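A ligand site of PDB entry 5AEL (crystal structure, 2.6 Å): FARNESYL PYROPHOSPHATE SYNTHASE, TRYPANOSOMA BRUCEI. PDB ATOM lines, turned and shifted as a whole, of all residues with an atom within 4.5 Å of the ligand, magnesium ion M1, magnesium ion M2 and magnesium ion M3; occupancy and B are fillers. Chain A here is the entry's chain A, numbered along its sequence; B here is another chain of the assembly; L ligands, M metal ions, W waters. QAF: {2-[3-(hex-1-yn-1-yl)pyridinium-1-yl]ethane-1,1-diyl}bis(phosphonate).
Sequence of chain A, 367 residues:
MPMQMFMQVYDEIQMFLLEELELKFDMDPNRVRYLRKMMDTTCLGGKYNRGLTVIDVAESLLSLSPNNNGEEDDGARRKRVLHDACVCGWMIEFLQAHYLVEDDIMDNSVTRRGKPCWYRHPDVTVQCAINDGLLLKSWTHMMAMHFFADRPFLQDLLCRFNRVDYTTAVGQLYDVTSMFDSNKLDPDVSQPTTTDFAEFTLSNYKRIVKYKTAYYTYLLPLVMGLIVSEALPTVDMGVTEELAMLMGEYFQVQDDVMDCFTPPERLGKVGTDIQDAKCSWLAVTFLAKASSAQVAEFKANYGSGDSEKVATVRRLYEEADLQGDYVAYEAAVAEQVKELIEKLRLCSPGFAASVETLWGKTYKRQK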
ATOM      1  N   HIS A  98     -17.720  -6.795 -17.183  1.00  0.00           N
ATOM      2  CA  HIS A  98     -18.065  -7.802 -16.169  1.00  0.00           C
ATOM      3  C   HIS A  98     -19.388  -7.475 -15.447  1.00  0.00           C
ATOM      4  O   HIS A  98     -20.330  -8.271 -15.453  1.00  0.00           O
ATOM      5  CB  HIS A  98     -16.898  -7.893 -15.183  1.00  0.00           C
ATOM      6  CG  HIS A  98     -17.280  -8.342 -13.817  1.00  0.00           C
ATOM      7  ND1 HIS A  98     -17.701  -9.623 -13.559  1.00  0.00           N
ATOM      8  CD2 HIS A  98     -17.239  -7.707 -12.619  1.00  0.00           C
ATOM      9  CE1 HIS A  98     -17.939  -9.745 -12.257  1.00  0.00           C
ATOM     10  NE2 HIS A  98     -17.683  -8.593 -11.679  1.00  0.00           N
ATOM     11  N   TYR A  99     -19.458  -6.280 -14.856  1.00  0.00           N
ATOM     12  CA  TYR A  99     -20.668  -5.860 -14.144  1.00  0.00           C
ATOM     13  C   TYR A  99     -21.922  -5.951 -14.998  1.00  0.00           C
ATOM     14  O   TYR A  99     -22.967  -6.394 -14.531  1.00  0.00           O
ATOM     15  CB  TYR A  99     -20.524  -4.439 -13.593  1.00  0.00           C
ATOM     16  CG  TYR A  99     -19.432  -4.171 -12.572  1.00  0.00           C
ATOM     17  CD1 TYR A  99     -18.895  -5.181 -11.781  1.00  0.00           C
ATOM     18  CD2 TYR A  99     -18.956  -2.873 -12.364  1.00  0.00           C
ATOM     19  CE1 TYR A  99     -17.888  -4.904 -10.851  1.00  0.00           C
ATOM     20  CE2 TYR A  99     -17.987  -2.581 -11.420  1.00  0.00           C
ATOM     21  CZ  TYR A  99     -17.465  -3.596 -10.676  1.00  0.00           C
ATOM     22  OH  TYR A  99     -16.493  -3.292  -9.753  1.00  0.00           O
ATOM     23  N   LEU A 100     -21.853  -5.521 -16.230  1.00  0.00           N
ATOM     24  CA  LEU A 100     -23.035  -5.612 -17.114  1.00  0.00           C
ATOM     25  C   LEU A 100     -23.510  -7.039 -17.468  1.00  0.00           C
ATOM     26  O   LEU A 100     -24.698  -7.320 -17.454  1.00  0.00           O
ATOM     27  CB  LEU A 100     -22.800  -4.803 -18.406  1.00  0.00           C
ATOM     28  CG  LEU A 100     -22.588  -3.327 -18.110  1.00  0.00           C
ATOM     29  CD1 LEU A 100     -22.625  -2.495 -19.386  1.00  0.00           C
ATOM     30  CD2 LEU A 100     -23.604  -2.793 -17.106  1.00  0.00           C
ATOM     31  N   ASP A 103     -25.089  -7.899 -14.201  1.00  0.00           N
ATOM     32  CA  ASP A 103     -26.248  -7.046 -13.910  1.00  0.00           C
ATOM     33  C   ASP A 103     -27.405  -7.477 -14.751  1.00  0.00           C
ATOM     34  O   ASP A 103     -28.504  -7.628 -14.230  1.00  0.00           O
ATOM     35  CB  ASP A 103     -25.970  -5.566 -14.168  1.00  0.00           C
ATOM     36  CG  ASP A 103     -27.206  -4.660 -13.868  1.00  0.00           C
ATOM     37  OD1 ASP A 103     -27.615  -4.441 -12.700  1.00  0.00           O
ATOM     38  OD2 ASP A 103     -27.763  -4.094 -14.838  1.00  0.00           O
ATOM     39  N   MET A 106     -28.993 -10.575 -13.320  1.00  0.00           N
ATOM     40  CA  MET A 106     -29.664 -10.122 -12.107  1.00  0.00           C
ATOM     41  C   MET A 106     -30.875  -9.230 -12.386  1.00  0.00           C
ATOM     42  O   MET A 106     -31.864  -9.357 -11.729  1.00  0.00           O
ATOM     43  CB  MET A 106     -28.699  -9.328 -11.255  1.00  0.00           C
ATOM     44  CG  MET A 106     -27.545 -10.118 -10.700  1.00  0.00           C
ATOM     45  SD  MET A 106     -26.655  -9.067  -9.537  1.00  0.00           S
ATOM     46  CE  MET A 106     -24.975  -9.683  -9.567  1.00  0.00           C
ATOM     47  N   ASP A 107     -30.796  -8.362 -13.376  1.00  0.00           N
ATOM     48  CA  ASP A 107     -31.889  -7.418 -13.674  1.00  0.00           C
ATOM     49  C   ASP A 107     -32.878  -8.013 -14.683  1.00  0.00           C
ATOM     50  O   ASP A 107     -33.840  -7.359 -15.097  1.00  0.00           O
ATOM     51  CB  ASP A 107     -31.303  -6.093 -14.240  1.00  0.00           C
ATOM     52  CG  ASP A 107     -30.548  -5.274 -13.179  1.00  0.00           C
ATOM     53  OD1 ASP A 107     -30.483  -5.732 -12.015  1.00  0.00           O
ATOM     54  OD2 ASP A 107     -30.046  -4.154 -13.512  1.00  0.00           O
ATOM     55  N   SER A 109     -32.623  -8.499 -17.929  1.00  0.00           N
ATOM     56  CA  SER A 109     -32.794  -7.576 -19.019  1.00  0.00           C
ATOM     57  C   SER A 109     -32.694  -8.377 -20.279  1.00  0.00           C
ATOM     58  O   SER A 109     -32.262  -9.543 -20.244  1.00  0.00           O
ATOM     59  CB  SER A 109     -31.690  -6.502 -19.028  1.00  0.00           C
ATOM     60  OG  SER A 109     -31.625  -5.791 -17.817  1.00  0.00           O
ATOM     61  N   ARG A 112     -28.971  -4.998 -24.755  1.00  0.00           N
ATOM     62  CA  ARG A 112     -27.839  -4.224 -24.239  1.00  0.00           C
ATOM     63  C   ARG A 112     -26.981  -3.820 -25.436  1.00  0.00           C
ATOM     64  O   ARG A 112     -26.570  -4.666 -26.252  1.00  0.00           O
ATOM     65  CB  ARG A 112     -27.043  -5.069 -23.228  1.00  0.00           C
ATOM     66  CG  ARG A 112     -25.610  -4.641 -22.889  1.00  0.00           C
ATOM     67  CD  ARG A 112     -25.534  -3.463 -21.913  1.00  0.00           C
ATOM     68  NE  ARG A 112     -25.912  -3.845 -20.550  1.00  0.00           N
ATOM     69  CZ  ARG A 112     -26.319  -3.000 -19.573  1.00  0.00           C
ATOM     70  NH1 ARG A 112     -26.399  -1.700 -19.733  1.00  0.00           N
ATOM     71  NH2 ARG A 112     -26.647  -3.488 -18.394  1.00  0.00           N
ATOM     72  N   LYS A 137     -13.745 -10.035 -15.325  1.00  0.00           N
ATOM     73  CA  LYS A 137     -13.138  -9.457 -14.132  1.00  0.00           C
ATOM     74  C   LYS A 137     -11.679  -9.867 -14.010  1.00  0.00           C
ATOM     75  O   LYS A 137     -10.837  -9.008 -13.832  1.00  0.00           O
ATOM     76  CB  LYS A 137     -13.903  -9.909 -12.894  1.00  0.00           C
ATOM     77  CG  LYS A 137     -13.617  -9.091 -11.658  1.00  0.00           C
ATOM     78  CD  LYS A 137     -14.405  -9.693 -10.501  1.00  0.00           C
ATOM     79  CE  LYS A 137     -14.516  -8.731  -9.349  1.00  0.00           C
ATOM     80  NZ  LYS A 137     -15.775  -7.929  -9.415  1.00  0.00           N
ATOM     81  N   ASP A 165     -14.132  -1.971  -6.692  1.00  0.00           N
ATOM     82  CA  ASP A 165     -14.843  -3.128  -7.157  1.00  0.00           C
ATOM     83  C   ASP A 165     -15.720  -3.671  -6.042  1.00  0.00           C
ATOM     84  O   ASP A 165     -16.908  -3.972  -6.229  1.00  0.00           O
ATOM     85  CB  ASP A 165     -13.844  -4.180  -7.549  1.00  0.00           C
ATOM     86  CG  ASP A 165     -14.484  -5.426  -8.091  1.00  0.00           C
ATOM     87  OD1 ASP A 165     -15.524  -5.338  -8.771  1.00  0.00           O
ATOM     88  OD2 ASP A 165     -13.918  -6.492  -7.836  1.00  0.00           O
ATOM     89  N   THR A 168     -18.695  -1.490  -5.431  1.00  0.00           N
ATOM     90  CA  THR A 168     -19.723  -1.698  -6.443  1.00  0.00           C
ATOM     91  C   THR A 168     -20.598  -2.906  -6.125  1.00  0.00           C
ATOM     92  O   THR A 168     -21.838  -2.837  -6.231  1.00  0.00           O
ATOM     93  CB  THR A 168     -19.093  -1.893  -7.824  1.00  0.00           C
ATOM     94  OG1 THR A 168     -18.029  -0.943  -8.013  1.00  0.00           O
ATOM     95  CG2 THR A 168     -20.138  -1.704  -8.881  1.00  0.00           C
ATOM     96  N   ALA A 169     -19.954  -3.994  -5.719  1.00  0.00           N
ATOM     97  CA  ALA A 169     -20.664  -5.197  -5.253  1.00  0.00           C
ATOM     98  C   ALA A 169     -21.617  -4.944  -4.073  1.00  0.00           C
ATOM     99  O   ALA A 169     -22.712  -5.492  -4.008  1.00  0.00           O
ATOM    100  CB  ALA A 169     -19.633  -6.236  -4.841  1.00  0.00           C
ATOM    101  N   GLN A 172     -24.416  -3.097  -5.310  1.00  0.00           N
ATOM    102  CA  GLN A 172     -25.328  -3.980  -6.003  1.00  0.00           C
ATOM    103  C   GLN A 172     -26.291  -4.732  -5.109  1.00  0.00           C
ATOM    104  O   GLN A 172     -27.427  -4.974  -5.497  1.00  0.00           O
ATOM    105  CB  GLN A 172     -24.586  -4.896  -6.942  1.00  0.00           C
ATOM    106  CG  GLN A 172     -24.774  -4.370  -8.344  1.00  0.00           C
ATOM    107  CD  GLN A 172     -25.915  -5.003  -9.018  1.00  0.00           C
ATOM    108  OE1 GLN A 172     -26.291  -6.069  -8.644  1.00  0.00           O
ATOM    109  NE2 GLN A 172     -26.455  -4.385 -10.013  1.00  0.00           N
ATOM    110  N   ASP A 175     -29.084  -2.430  -4.336  1.00  0.00           N
ATOM    111  CA  ASP A 175     -30.029  -2.446  -5.469  1.00  0.00           C
ATOM    112  C   ASP A 175     -30.924  -3.680  -5.492  1.00  0.00           C
ATOM    113  O   ASP A 175     -32.128  -3.615  -5.734  1.00  0.00           O
ATOM    114  CB  ASP A 175     -29.207  -2.351  -6.789  1.00  0.00           C
ATOM    115  CG  ASP A 175     -30.079  -2.432  -8.060  1.00  0.00           C
ATOM    116  OD1 ASP A 175     -30.621  -3.506  -8.411  1.00  0.00           O
ATOM    117  OD2 ASP A 175     -30.149  -1.426  -8.773  1.00  0.00           O
ATOM    118  N   LYS A 212     -23.068   1.731  -6.011  1.00  0.00           N
ATOM    119  CA  LYS A 212     -23.168   0.863  -7.190  1.00  0.00           C
ATOM    120  C   LYS A 212     -22.711   1.551  -8.456  1.00  0.00           C
ATOM    121  O   LYS A 212     -22.447   0.883  -9.421  1.00  0.00           O
ATOM    122  CB  LYS A 212     -24.616   0.373  -7.443  1.00  0.00           C
ATOM    123  CG  LYS A 212     -25.491   1.344  -8.247  1.00  0.00           C
ATOM    124  CD  LYS A 212     -26.890   0.776  -8.484  1.00  0.00           C
ATOM    125  CE  LYS A 212     -27.828   1.686  -9.296  1.00  0.00           C
ATOM    126  NZ  LYS A 212     -28.938   0.880  -9.905  1.00  0.00           N
ATOM    127  N   THR A 213     -22.690   2.871  -8.480  1.00  0.00           N
ATOM    128  CA  THR A 213     -22.306   3.570  -9.696  1.00  0.00           C
ATOM    129  C   THR A 213     -21.187   4.649  -9.526  1.00  0.00           C
ATOM    130  O   THR A 213     -20.278   4.699 -10.340  1.00  0.00           O
ATOM    131  CB  THR A 213     -23.554   4.189 -10.342  1.00  0.00           C
ATOM    132  OG1 THR A 213     -24.492   3.159 -10.630  1.00  0.00           O
ATOM    133  CG2 THR A 213     -23.226   4.941 -11.624  1.00  0.00           C
ATOM    134  N   TYR A 216     -16.954   3.532  -9.196  1.00  0.00           N
ATOM    135  CA  TYR A 216     -16.310   3.001 -10.381  1.00  0.00           C
ATOM    136  C   TYR A 216     -16.498   3.843 -11.597  1.00  0.00           C
ATOM    137  O   TYR A 216     -15.667   3.816 -12.498  1.00  0.00           O
ATOM    138  CB  TYR A 216     -16.730   1.575 -10.662  1.00  0.00           C
ATOM    139  CG  TYR A 216     -17.918   1.372 -11.551  1.00  0.00           C
ATOM    140  CD1 TYR A 216     -19.195   1.274 -11.027  1.00  0.00           C
ATOM    141  CD2 TYR A 216     -17.753   1.169 -12.898  1.00  0.00           C
ATOM    142  CE1 TYR A 216     -20.262   0.992 -11.858  1.00  0.00           C
ATOM    143  CE2 TYR A 216     -18.818   0.932 -13.731  1.00  0.00           C
ATOM    144  CZ  TYR A 216     -20.051   0.831 -13.214  1.00  0.00           C
ATOM    145  OH  TYR A 216     -21.080   0.587 -14.051  1.00  0.00           O
ATOM    146  N   GLN A 252     -26.590   8.389 -12.312  1.00  0.00           N
ATOM    147  CA  GLN A 252     -27.565   7.313 -12.057  1.00  0.00           C
ATOM    148  C   GLN A 252     -29.013   7.803 -12.093  1.00  0.00           C
ATOM    149  O   GLN A 252     -29.901   7.137 -12.658  1.00  0.00           O
ATOM    150  CB  GLN A 252     -27.259   6.588 -10.742  1.00  0.00           C
ATOM    151  CG  GLN A 252     -27.870   5.225 -10.585  1.00  0.00           C
ATOM    152  CD  GLN A 252     -27.625   4.323 -11.770  1.00  0.00           C
ATOM    153  OE1 GLN A 252     -26.453   4.100 -12.173  1.00  0.00           O
ATOM    154  NE2 GLN A 252     -28.730   3.769 -12.340  1.00  0.00           N
ATOM    155  N   ASP A 255     -29.697   7.813 -15.567  1.00  0.00           N
ATOM    156  CA  ASP A 255     -29.906   6.406 -15.999  1.00  0.00           C
ATOM    157  C   ASP A 255     -31.319   5.989 -15.685  1.00  0.00           C
ATOM    158  O   ASP A 255     -32.012   5.456 -16.535  1.00  0.00           O
ATOM    159  CB  ASP A 255     -28.960   5.403 -15.324  1.00  0.00           C
ATOM    160  CG  ASP A 255     -29.054   3.994 -15.944  1.00  0.00           C
ATOM    161  OD1 ASP A 255     -28.789   3.942 -17.140  1.00  0.00           O
ATOM    162  OD2 ASP A 255     -29.415   2.964 -15.301  1.00  0.00           O
ATOM    163  N   ASP A 259     -34.373   4.992 -18.382  1.00  0.00           N
ATOM    164  CA  ASP A 259     -34.853   3.623 -18.324  1.00  0.00           C
ATOM    165  C   ASP A 259     -36.320   3.649 -18.589  1.00  0.00           C
ATOM    166  O   ASP A 259     -36.851   2.769 -19.233  1.00  0.00           O
ATOM    167  CB  ASP A 259     -34.618   2.997 -16.973  1.00  0.00           C
ATOM    168  CG  ASP A 259     -34.681   1.517 -17.028  1.00  0.00           C
ATOM    169  OD1 ASP A 259     -33.638   0.910 -17.436  1.00  0.00           O
ATOM    170  OD2 ASP A 259     -35.730   0.964 -16.616  1.00  0.00           O
ATOM    171  N   LYS A 269     -31.075  -0.389 -25.205  1.00  0.00           N
ATOM    172  CA  LYS A 269     -31.556  -1.356 -24.235  1.00  0.00           C
ATOM    173  C   LYS A 269     -32.967  -1.054 -23.793  1.00  0.00           C
ATOM    174  O   LYS A 269     -33.394   0.113 -23.798  1.00  0.00           O
ATOM    175  CB  LYS A 269     -30.593  -1.453 -23.019  1.00  0.00           C
ATOM    176  CG  LYS A 269     -30.500  -0.178 -22.222  1.00  0.00           C
ATOM    177  CD  LYS A 269     -29.489  -0.242 -21.104  1.00  0.00           C
ATOM    178  CE  LYS A 269     -29.807   0.805 -20.048  1.00  0.00           C
ATOM    179  NZ  LYS A 269     -28.546   1.417 -19.512  1.00  0.00           N
ATOM    180  N   ASP A 273     -36.593  -1.406 -14.852  1.00  0.00           N
ATOM    181  CA  ASP A 273     -36.662  -0.899 -13.451  1.00  0.00           C
ATOM    182  C   ASP A 273     -38.084  -1.029 -12.887  1.00  0.00           C
ATOM    183  O   ASP A 273     -38.317  -1.519 -11.741  1.00  0.00           O
ATOM    184  CB  ASP A 273     -36.213   0.564 -13.368  1.00  0.00           C
ATOM    185  CG  ASP A 273     -34.724   0.774 -13.704  1.00  0.00           C
ATOM    186  OD1 ASP A 273     -33.920  -0.205 -13.728  1.00  0.00           O
ATOM    187  OD2 ASP A 273     -34.359   1.975 -13.910  1.00  0.00           O
ATOM    188  N   LYS A 278     -37.599  -1.799  -9.017  1.00  0.00           N
ATOM    189  CA  LYS A 278     -36.370  -1.201  -8.516  1.00  0.00           C
ATOM    190  C   LYS A 278     -36.646   0.066  -7.769  1.00  0.00           C
ATOM    191  O   LYS A 278     -37.569   0.790  -8.100  1.00  0.00           O
ATOM    192  CB  LYS A 278     -35.375  -0.890  -9.668  1.00  0.00           C
ATOM    193  CG  LYS A 278     -34.790  -2.132 -10.277  1.00  0.00           C
ATOM    194  CD  LYS A 278     -33.750  -2.791  -9.378  1.00  0.00           C
ATOM    195  CE  LYS A 278     -33.365  -4.166  -9.873  1.00  0.00           C
ATOM    196  NZ  LYS A 278     -32.730  -4.185 -11.222  1.00  0.00           N
ATOM    197  N   ASN B 131     -24.525 -12.235  -6.712  1.00  0.00           N
ATOM    198  CA  ASN B 131     -23.802 -11.105  -6.177  1.00  0.00           C
ATOM    199  C   ASN B 131     -23.167 -11.414  -4.835  1.00  0.00           C
ATOM    200  O   ASN B 131     -22.028 -11.004  -4.586  1.00  0.00           O
ATOM    201  CB  ASN B 131     -24.735  -9.912  -6.023  1.00  0.00           C
ATOM    202  CG  ASN B 131     -23.978  -8.610  -5.843  1.00  0.00           C
ATOM    203  OD1 ASN B 131     -23.265  -8.153  -6.770  1.00  0.00           O
ATOM    204  ND2 ASN B 131     -24.090  -8.031  -4.652  1.00  0.00           N
ATOM    205  N   LEU B 134     -20.018 -12.775  -5.416  1.00  0.00           N
ATOM    206  CA  LEU B 134     -19.014 -11.762  -5.732  1.00  0.00           C
ATOM    207  C   LEU B 134     -18.475 -10.997  -4.518  1.00  0.00           C
ATOM    208  O   LEU B 134     -17.286 -10.672  -4.473  1.00  0.00           O
ATOM    209  CB  LEU B 134     -19.591 -10.756  -6.720  1.00  0.00           C
ATOM    210  CG  LEU B 134     -20.032 -11.335  -8.057  1.00  0.00           C
ATOM    211  CD1 LEU B 134     -20.633 -10.212  -8.865  1.00  0.00           C
ATOM    212  CD2 LEU B 134     -18.885 -11.935  -8.834  1.00  0.00           C
HETATM  213  C01 QAF L   1     -19.848  -6.743  -8.113  1.00  0.00           C
HETATM  214  C02 QAF L   1     -20.873  -6.981  -9.194  1.00  0.00           C
HETATM  215  C03 QAF L   1     -21.635  -5.726  -9.602  1.00  0.00           C
HETATM  216  C04 QAF L   1     -22.695  -6.045 -10.705  1.00  0.00           C
HETATM  217  C05 QAF L   1     -23.212  -4.714 -11.170  1.00  0.00           C
HETATM  218  C06 QAF L   1     -23.627  -3.602 -11.528  1.00  0.00           C
HETATM  219  C07 QAF L   1     -24.128  -2.276 -11.975  1.00  0.00           C
HETATM  220  C08 QAF L   1     -23.853  -1.095 -11.269  1.00  0.00           C
HETATM  221  C09 QAF L   1     -24.359   0.109 -11.740  1.00  0.00           C
HETATM  222  C10 QAF L   1     -25.130   0.137 -12.909  1.00  0.00           C
HETATM  223  N11 QAF L   1     -25.373  -1.053 -13.579  1.00  0.00           N
HETATM  224  C12 QAF L   1     -26.124  -1.136 -14.795  1.00  0.00           C
HETATM  225  C13 QAF L   1     -27.362  -0.237 -14.879  1.00  0.00           C
HETATM  226  P14 QAF L   1     -28.133  -0.443 -16.492  1.00  0.00           P
HETATM  227  O15 QAF L   1     -27.280  -1.214 -17.371  1.00  0.00           O
HETATM  228  O16 QAF L   1     -28.318   0.958 -17.036  1.00  0.00           O
HETATM  229  O17 QAF L   1     -29.428  -1.176 -16.462  1.00  0.00           O
HETATM  230  P18 QAF L   1     -28.588  -0.477 -13.518  1.00  0.00           P
HETATM  231  O19 QAF L   1     -29.710   0.446 -13.992  1.00  0.00           O
HETATM  232  O20 QAF L   1     -28.891  -1.967 -13.306  1.00  0.00           O
HETATM  233  O21 QAF L   1     -27.907   0.023 -12.280  1.00  0.00           O
HETATM  234  C22 QAF L   1     -24.861  -2.221 -13.110  1.00  0.00           C
HETATM  235 MG    MG M   1     -29.473  -2.960 -15.293  1.00  0.00          MG
HETATM  236 MG    MG M   2     -30.881   1.179 -15.654  1.00  0.00          MG
HETATM  237 MG    MG M   3     -28.910  -3.159 -11.511  1.00  0.00          MG
HETATM  238  O   HOH W   1     -29.537  -4.948 -16.505  1.00  0.00           O
HETATM  239  O   HOH W   2     -31.659  -2.051 -15.338  1.00  0.00           O
HETATM  240  O   HOH W   3     -30.902  -0.806 -11.882  1.00  0.00           O
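NZ of Lys 269 is in salt-bridge range of O16 of the ligand (2.5 Å).
NH1 of Arg 112 lies within salt-bridge range of O15 of the ligand (2.6 Å).
The side-chain amino group (NZ) of Lys 212 is in salt-bridge range of an oxygen (O21) of the ligand, 2.7 Å away.
The side-chain amide oxygen of Gln 172 lies close to the side-chain sulfur of Met 106 (3.1 Å).
The side-chain carboxylate (OD2) of Asp 259 lies within hydrogen-bond range of the backbone NH (N) of Asp 273.
OD1 of Asp 255 lies within salt-bridge range of NZ of Lys 269 (3.5 Å).
The side-chain amide oxygen of Gln 252 sits at hydrogen-bond distance from the side-chain hydroxyl of Thr 213 (2.7 Å).
OH of Tyr 99 sits at hydrogen-bond distance from OD1 of Asp 165 (2.5 Å).
The backbone carbonyl oxygen (O) of Asp 273 is in hydrogen-bond range of the backbone NH (N) of Lys 278, 2.8 Å away.
The side-chain carboxylate of Asp 103 lies close to the side-chain amide nitrogen of Gln 172, 2.9 Å away.
NZ of Lys 278 lies within salt-bridge range of OD1 of Asp 107 (2.8 Å).
Residues that only touch the ligand: Tyr 99, Leu 100, Ala 169, Gln 172, Thr 213, Gln 252, Asn 131 of chain B and Leu 134 of chain B.
Hydrophobic or aromatic side chains within 4 Å of the ligand: Tyr 99, Leu 100, Ala 169 and Leu 134 of chain B.
Within 4 Å of the ligand: Tyr 99, Leu 100, Asp 103, Asp 107, Arg 112, Ala 169, Gln 172, Lys 212, Thr 213, Gln 252, Asp 255, Lys 269, Asn 131 of chain B and Leu 134 of chain B.
Of the 25 residues printed, 2 come within 4 Å of magnesium ion M1.
The nearest printed residue that does not touch magnesium ion M1 is Arg 112 (4.2 Å).
Asp 259 touches magnesium ion M2.
Asp 273 touches magnesium ion M2.
Residues that only touch magnesium ion M3: Gln 172, Asp 175 and Lys 278.
Of the 25 residues printed, 5 come within 4 Å of magnesium ion M3.
Along chain A the residues within 4 Å of magnesium ion M3 span positions 103 to 278.
Magnesium ion M1 is bound by the side-chain carboxylate (OD2) of Asp 103, an oxygen (O17) of the ligand, the side-chain carboxylate (OD2) of Asp 107, an oxygen (O20) of the ligand, water W1 and water W2.
Magnesium ion M1 has six donor atoms within binding distance.
O19 of the ligand binds magnesium ion M2.
Magnesium ion M2 is bound by OD2 of Asp 255.
O20 of the ligand binds magnesium ion M3 (2.2 Å).
OD1 of Asp 103 is bound to magnesium ion M3, 2.2 Å away.
The side-chain carboxylate (OD2) of Asp 107 binds magnesium ion M3, at 2.5 Å.
Water W3 lies within hydrogen-bond range of O21 of the ligand (3.1 Å), NZ of Lys 212 (3.3 Å) and OD2 of Asp 175 (3.3 Å).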
